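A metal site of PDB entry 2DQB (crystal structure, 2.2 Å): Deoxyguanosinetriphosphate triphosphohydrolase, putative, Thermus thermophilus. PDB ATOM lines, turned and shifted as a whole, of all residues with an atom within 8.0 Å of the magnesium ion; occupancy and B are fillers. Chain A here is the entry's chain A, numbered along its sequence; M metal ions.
The magnesium ion is bound by OD1 of Asp 196 (2.2 Å), OD2 of Asp 109 (2.3 Å) and NE2 of His 79 (2.4 Å).
His 108 touches the magnesium ion.
CE1 of Tyr 200 touches the magnesium ion, 3.2 Å away.
The nearest printed residue that does not touch the magnesium ion is Gln 63 (4.02 Å).
A ring nitrogen (NE2) of His 108 sits close to the backbone carbonyl oxygen (O) of Ala 105 (3.3 Å).
A ring nitrogen (ND1) of His 79 lies within hydrogen-bond range of the guanidinium group (NH2) of Arg 74, 3.0 Å away.
ND1 of His 112 sits at hydrogen-bond distance from OD1 of Asp 109 (3.4 Å).
The side-chain hydroxyl of Tyr 200 is in hydrogen-bond range of the side-chain amide nitrogen of Gln 63.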
ATOM      1  N   GLN A  63      -4.841   4.792  -9.164  1.00  0.00           N
ATOM      2  CA  GLN A  63      -5.948   3.847  -9.342  1.00  0.00           C
ATOM      3  C   GLN A  63      -6.806   4.017  -8.078  1.00  0.00           C
ATOM      4  O   GLN A  63      -6.275   4.036  -6.960  1.00  0.00           O
ATOM      5  CB  GLN A  63      -5.387   2.410  -9.401  1.00  0.00           C
ATOM      6  CG  GLN A  63      -6.247   1.360 -10.122  1.00  0.00           C
ATOM      7  CD  GLN A  63      -5.986   1.325 -11.621  1.00  0.00           C
ATOM      8  OE1 GLN A  63      -4.855   1.464 -12.082  1.00  0.00           O
ATOM      9  NE2 GLN A  63      -7.046   1.106 -12.396  1.00  0.00           N
ATOM     10  N   ARG A  74      -1.142   2.341  -4.856  1.00  0.00           N
ATOM     11  CA  ARG A  74      -0.665   1.745  -6.103  1.00  0.00           C
ATOM     12  C   ARG A  74      -0.157   2.706  -7.187  1.00  0.00           C
ATOM     13  O   ARG A  74       1.059   3.000  -7.250  1.00  0.00           O
ATOM     14  CB  ARG A  74      -1.740   0.842  -6.727  1.00  0.00           C
ATOM     15  CG  ARG A  74      -1.781  -0.554  -6.122  1.00  0.00           C
ATOM     16  CD  ARG A  74      -2.573  -1.520  -7.019  1.00  0.00           C
ATOM     17  NE  ARG A  74      -3.937  -1.061  -7.273  1.00  0.00           N
ATOM     18  CZ  ARG A  74      -4.792  -1.687  -8.080  1.00  0.00           C
ATOM     19  NH1 ARG A  74      -6.007  -1.204  -8.263  1.00  0.00           N
ATOM     20  NH2 ARG A  74      -4.423  -2.789  -8.717  1.00  0.00           N
ATOM     21  N   ARG A  76      -1.716   3.948 -11.420  1.00  0.00           N
ATOM     22  CA  ARG A  76      -2.183   3.231 -12.600  1.00  0.00           C
ATOM     23  C   ARG A  76      -1.060   2.358 -13.151  1.00  0.00           C
ATOM     24  O   ARG A  76      -1.335   1.282 -13.642  1.00  0.00           O
ATOM     25  CB  ARG A  76      -2.699   4.192 -13.655  1.00  0.00           C
ATOM     26  CG  ARG A  76      -4.106   4.778 -13.367  1.00  0.00           C
ATOM     27  CD  ARG A  76      -4.673   5.431 -14.637  1.00  0.00           C
ATOM     28  NE  ARG A  76      -6.043   5.942 -14.510  1.00  0.00           N
ATOM     29  CZ  ARG A  76      -6.375   7.088 -13.906  1.00  0.00           C
ATOM     30  NH1 ARG A  76      -7.649   7.455 -13.854  1.00  0.00           N
ATOM     31  NH2 ARG A  76      -5.453   7.864 -13.348  1.00  0.00           N
ATOM     32  N   HIS A  79      -0.893  -0.962 -11.281  1.00  0.00           N
ATOM     33  CA  HIS A  79      -2.040  -1.754 -11.693  1.00  0.00           C
ATOM     34  C   HIS A  79      -1.760  -2.502 -12.997  1.00  0.00           C
ATOM     35  O   HIS A  79      -1.897  -3.724 -13.085  1.00  0.00           O
ATOM     36  CB  HIS A  79      -3.273  -0.848 -11.860  1.00  0.00           C
ATOM     37  CG  HIS A  79      -4.482  -1.566 -12.349  1.00  0.00           C
ATOM     38  ND1 HIS A  79      -5.117  -2.533 -11.593  1.00  0.00           N
ATOM     39  CD2 HIS A  79      -5.146  -1.514 -13.524  1.00  0.00           C
ATOM     40  CE1 HIS A  79      -6.128  -3.040 -12.287  1.00  0.00           C
ATOM     41  NE2 HIS A  79      -6.163  -2.429 -13.462  1.00  0.00           N
ATOM     42  N   THR A  80      -1.398  -1.735 -14.010  1.00  0.00           N
ATOM     43  CA  THR A  80      -1.067  -2.226 -15.351  1.00  0.00           C
ATOM     44  C   THR A  80      -0.045  -3.354 -15.294  1.00  0.00           C
ATOM     45  O   THR A  80      -0.243  -4.426 -15.877  1.00  0.00           O
ATOM     46  CB  THR A  80      -0.502  -1.045 -16.168  1.00  0.00           C
ATOM     47  OG1 THR A  80      -1.554  -0.102 -16.391  1.00  0.00           O
ATOM     48  CG2 THR A  80       0.142  -1.505 -17.507  1.00  0.00           C
ATOM     49  N   VAL A  83      -1.760  -6.243 -14.130  1.00  0.00           N
ATOM     50  CA  VAL A  83      -2.653  -6.840 -15.127  1.00  0.00           C
ATOM     51  C   VAL A  83      -1.771  -7.593 -16.145  1.00  0.00           C
ATOM     52  O   VAL A  83      -2.140  -8.665 -16.629  1.00  0.00           O
ATOM     53  CB  VAL A  83      -3.521  -5.781 -15.858  1.00  0.00           C
ATOM     54  CG1 VAL A  83      -4.296  -6.433 -17.018  1.00  0.00           C
ATOM     55  CG2 VAL A  83      -4.495  -5.142 -14.888  1.00  0.00           C
ATOM     56  N   ALA A 105      -2.323  -5.513 -22.415  1.00  0.00           N
ATOM     57  CA  ALA A 105      -2.356  -5.158 -20.986  1.00  0.00           C
ATOM     58  C   ALA A 105      -1.636  -3.839 -20.713  1.00  0.00           C
ATOM     59  O   ALA A 105      -2.076  -3.041 -19.877  1.00  0.00           O
ATOM     60  CB  ALA A 105      -1.736  -6.272 -20.131  1.00  0.00           C
ATOM     61  N   HIS A 108      -4.222  -0.944 -22.783  1.00  0.00           N
ATOM     62  CA  HIS A 108      -5.657  -0.779 -22.517  1.00  0.00           C
ATOM     63  C   HIS A 108      -6.060   0.360 -21.574  1.00  0.00           C
ATOM     64  O   HIS A 108      -7.120   0.931 -21.729  1.00  0.00           O
ATOM     65  CB  HIS A 108      -6.273  -2.091 -22.012  1.00  0.00           C
ATOM     66  CG  HIS A 108      -5.984  -2.359 -20.570  1.00  0.00           C
ATOM     67  ND1 HIS A 108      -6.965  -2.426 -19.614  1.00  0.00           N
ATOM     68  CD2 HIS A 108      -4.813  -2.544 -19.915  1.00  0.00           C
ATOM     69  CE1 HIS A 108      -6.418  -2.626 -18.430  1.00  0.00           C
ATOM     70  NE2 HIS A 108      -5.104  -2.695 -18.581  1.00  0.00           N
ATOM     71  N   ASP A 109      -5.237   0.699 -20.586  1.00  0.00           N
ATOM     72  CA  ASP A 109      -5.615   1.776 -19.672  1.00  0.00           C
ATOM     73  C   ASP A 109      -4.969   3.117 -19.901  1.00  0.00           C
ATOM     74  O   ASP A 109      -4.998   3.965 -19.022  1.00  0.00           O
ATOM     75  CB  ASP A 109      -5.389   1.366 -18.226  1.00  0.00           C
ATOM     76  CG  ASP A 109      -6.579   0.632 -17.632  1.00  0.00           C
ATOM     77  OD1 ASP A 109      -7.684   0.736 -18.203  1.00  0.00           O
ATOM     78  OD2 ASP A 109      -6.412  -0.027 -16.583  1.00  0.00           O
ATOM     79  N   HIS A 112      -7.294   6.694 -19.815  1.00  0.00           N
ATOM     80  CA  HIS A 112      -7.970   7.190 -18.643  1.00  0.00           C
ATOM     81  C   HIS A 112      -7.517   8.601 -18.336  1.00  0.00           C
ATOM     82  O   HIS A 112      -6.354   8.958 -18.515  1.00  0.00           O
ATOM     83  CB  HIS A 112      -7.689   6.294 -17.429  1.00  0.00           C
ATOM     84  CG  HIS A 112      -8.744   5.273 -17.167  1.00  0.00           C
ATOM     85  ND1 HIS A 112      -8.494   3.905 -17.197  1.00  0.00           N
ATOM     86  CD2 HIS A 112     -10.046   5.398 -16.800  1.00  0.00           C
ATOM     87  CE1 HIS A 112      -9.592   3.255 -16.866  1.00  0.00           C
ATOM     88  NE2 HIS A 112     -10.547   4.138 -16.616  1.00  0.00           N
ATOM     89  N   HIS A 117     -11.050   6.629 -12.601  1.00  0.00           N
ATOM     90  CA  HIS A 117     -12.436   6.363 -13.011  1.00  0.00           C
ATOM     91  C   HIS A 117     -13.433   7.484 -12.788  1.00  0.00           C
ATOM     92  O   HIS A 117     -14.357   7.666 -13.594  1.00  0.00           O
ATOM     93  CB  HIS A 117     -12.935   5.057 -12.389  1.00  0.00           C
ATOM     94  CG  HIS A 117     -12.972   3.920 -13.356  1.00  0.00           C
ATOM     95  ND1 HIS A 117     -14.006   3.722 -14.241  1.00  0.00           N
ATOM     96  CD2 HIS A 117     -12.051   2.959 -13.638  1.00  0.00           C
ATOM     97  CE1 HIS A 117     -13.725   2.695 -15.029  1.00  0.00           C
ATOM     98  NE2 HIS A 117     -12.543   2.214 -14.679  1.00  0.00           N
ATOM     99  N   HIS A 135     -12.791   5.794 -22.000  1.00  0.00           N
ATOM    100  CA  HIS A 135     -11.366   5.488 -21.878  1.00  0.00           C
ATOM    101  C   HIS A 135     -10.742   4.500 -22.849  1.00  0.00           C
ATOM    102  O   HIS A 135      -9.539   4.555 -23.089  1.00  0.00           O
ATOM    103  CB  HIS A 135     -11.017   5.104 -20.432  1.00  0.00           C
ATOM    104  CG  HIS A 135     -11.382   3.691 -20.072  1.00  0.00           C
ATOM    105  ND1 HIS A 135     -10.433   2.710 -19.858  1.00  0.00           N
ATOM    106  CD2 HIS A 135     -12.586   3.104 -19.879  1.00  0.00           C
ATOM    107  CE1 HIS A 135     -11.039   1.581 -19.559  1.00  0.00           C
ATOM    108  NE2 HIS A 135     -12.347   1.786 -19.566  1.00  0.00           N
ATOM    109  N   HIS A 169     -11.603  -6.087 -26.271  1.00  0.00           N
ATOM    110  CA  HIS A 169     -11.488  -6.611 -24.917  1.00  0.00           C
ATOM    111  C   HIS A 169     -12.467  -5.747 -24.120  1.00  0.00           C
ATOM    112  O   HIS A 169     -12.653  -4.567 -24.457  1.00  0.00           O
ATOM    113  CB  HIS A 169     -10.050  -6.449 -24.392  1.00  0.00           C
ATOM    114  CG  HIS A 169      -9.814  -5.163 -23.644  1.00  0.00           C
ATOM    115  ND1 HIS A 169      -9.838  -5.094 -22.273  1.00  0.00           N
ATOM    116  CD2 HIS A 169      -9.561  -3.909 -24.084  1.00  0.00           C
ATOM    117  CE1 HIS A 169      -9.627  -3.848 -21.889  1.00  0.00           C
ATOM    118  NE2 HIS A 169      -9.447  -3.106 -22.974  1.00  0.00           N
ATOM    119  N   GLU A 170     -13.104  -6.314 -23.100  1.00  0.00           N
ATOM    120  CA  GLU A 170     -14.056  -5.520 -22.327  1.00  0.00           C
ATOM    121  C   GLU A 170     -15.239  -5.185 -23.238  1.00  0.00           C
ATOM    122  O   GLU A 170     -15.485  -4.024 -23.565  1.00  0.00           O
ATOM    123  CB  GLU A 170     -13.344  -4.241 -21.816  1.00  0.00           C
ATOM    124  CG  GLU A 170     -14.201  -3.204 -21.088  1.00  0.00           C
ATOM    125  CD  GLU A 170     -13.376  -2.014 -20.567  1.00  0.00           C
ATOM    126  OE1 GLU A 170     -13.967  -0.944 -20.294  1.00  0.00           O
ATOM    127  OE2 GLU A 170     -12.129  -2.134 -20.426  1.00  0.00           O
ATOM    128  N   VAL A 192      -6.981 -10.440 -21.254  1.00  0.00           N
ATOM    129  CA  VAL A 192      -6.586  -9.216 -20.612  1.00  0.00           C
ATOM    130  C   VAL A 192      -7.746  -8.621 -19.791  1.00  0.00           C
ATOM    131  O   VAL A 192      -7.568  -8.235 -18.644  1.00  0.00           O
ATOM    132  CB  VAL A 192      -6.081  -8.162 -21.603  1.00  0.00           C
ATOM    133  CG1 VAL A 192      -5.907  -6.836 -20.890  1.00  0.00           C
ATOM    134  CG2 VAL A 192      -4.736  -8.597 -22.206  1.00  0.00           C
ATOM    135  N   ASP A 193      -8.950  -8.546 -20.362  1.00  0.00           N
ATOM    136  CA  ASP A 193     -10.030  -7.959 -19.600  1.00  0.00           C
ATOM    137  C   ASP A 193     -10.285  -8.732 -18.334  1.00  0.00           C
ATOM    138  O   ASP A 193     -10.540  -8.144 -17.282  1.00  0.00           O
ATOM    139  CB  ASP A 193     -11.328  -7.871 -20.387  1.00  0.00           C
ATOM    140  CG  ASP A 193     -12.397  -7.061 -19.646  1.00  0.00           C
ATOM    141  OD1 ASP A 193     -12.184  -5.843 -19.428  1.00  0.00           O
ATOM    142  OD2 ASP A 193     -13.427  -7.638 -19.255  1.00  0.00           O
ATOM    143  N   SER A 195      -8.126 -10.456 -16.633  1.00  0.00           N
ATOM    144  CA  SER A 195      -7.007 -10.205 -15.742  1.00  0.00           C
ATOM    145  C   SER A 195      -7.182  -8.870 -15.080  1.00  0.00           C
ATOM    146  O   SER A 195      -6.843  -8.689 -13.914  1.00  0.00           O
ATOM    147  CB  SER A 195      -5.684 -10.231 -16.507  1.00  0.00           C
ATOM    148  OG  SER A 195      -5.459 -11.514 -17.056  1.00  0.00           O
ATOM    149  N   ASP A 196      -7.709  -7.916 -15.833  1.00  0.00           N
ATOM    150  CA  ASP A 196      -7.936  -6.582 -15.302  1.00  0.00           C
ATOM    151  C   ASP A 196      -8.856  -6.703 -14.060  1.00  0.00           C
ATOM    152  O   ASP A 196      -8.546  -6.178 -12.997  1.00  0.00           O
ATOM    153  CB  ASP A 196      -8.603  -5.733 -16.406  1.00  0.00           C
ATOM    154  CG  ASP A 196      -8.649  -4.265 -16.068  1.00  0.00           C
ATOM    155  OD1 ASP A 196      -7.917  -3.817 -15.165  1.00  0.00           O
ATOM    156  OD2 ASP A 196      -9.412  -3.533 -16.735  1.00  0.00           O
ATOM    157  N   ALA A 197      -9.985  -7.397 -14.203  1.00  0.00           N
ATOM    158  CA  ALA A 197     -10.926  -7.574 -13.097  1.00  0.00           C
ATOM    159  C   ALA A 197     -10.263  -8.261 -11.914  1.00  0.00           C
ATOM    160  O   ALA A 197     -10.404  -7.826 -10.780  1.00  0.00           O
ATOM    161  CB  ALA A 197     -12.130  -8.380 -13.549  1.00  0.00           C
ATOM    162  N   ALA A 199      -7.020  -8.480 -11.178  1.00  0.00           N
ATOM    163  CA  ALA A 199      -6.054  -7.553 -10.600  1.00  0.00           C
ATOM    164  C   ALA A 199      -6.692  -6.471  -9.723  1.00  0.00           C
ATOM    165  O   ALA A 199      -6.215  -6.189  -8.627  1.00  0.00           O
ATOM    166  CB  ALA A 199      -5.265  -6.911 -11.697  1.00  0.00           C
ATOM    167  N   TYR A 200      -7.758  -5.851 -10.222  1.00  0.00           N
ATOM    168  CA  TYR A 200      -8.452  -4.796  -9.510  1.00  0.00           C
ATOM    169  C   TYR A 200      -8.838  -5.258  -8.117  1.00  0.00           C
ATOM    170  O   TYR A 200      -8.559  -4.596  -7.118  1.00  0.00           O
ATOM    171  CB  TYR A 200      -9.735  -4.397 -10.256  1.00  0.00           C
ATOM    172  CG  TYR A 200      -9.713  -3.067 -10.978  1.00  0.00           C
ATOM    173  CD1 TYR A 200      -9.772  -3.014 -12.366  1.00  0.00           C
ATOM    174  CD2 TYR A 200      -9.668  -1.862 -10.264  1.00  0.00           C
ATOM    175  CE1 TYR A 200      -9.794  -1.785 -13.038  1.00  0.00           C
ATOM    176  CE2 TYR A 200      -9.689  -0.620 -10.919  1.00  0.00           C
ATOM    177  CZ  TYR A 200      -9.752  -0.600 -12.314  1.00  0.00           C
ATOM    178  OH  TYR A 200      -9.767   0.596 -13.002  1.00  0.00           O
HETATM  179 MG    MG M   1      -7.475  -1.651 -15.289  1.00  0.00          MG
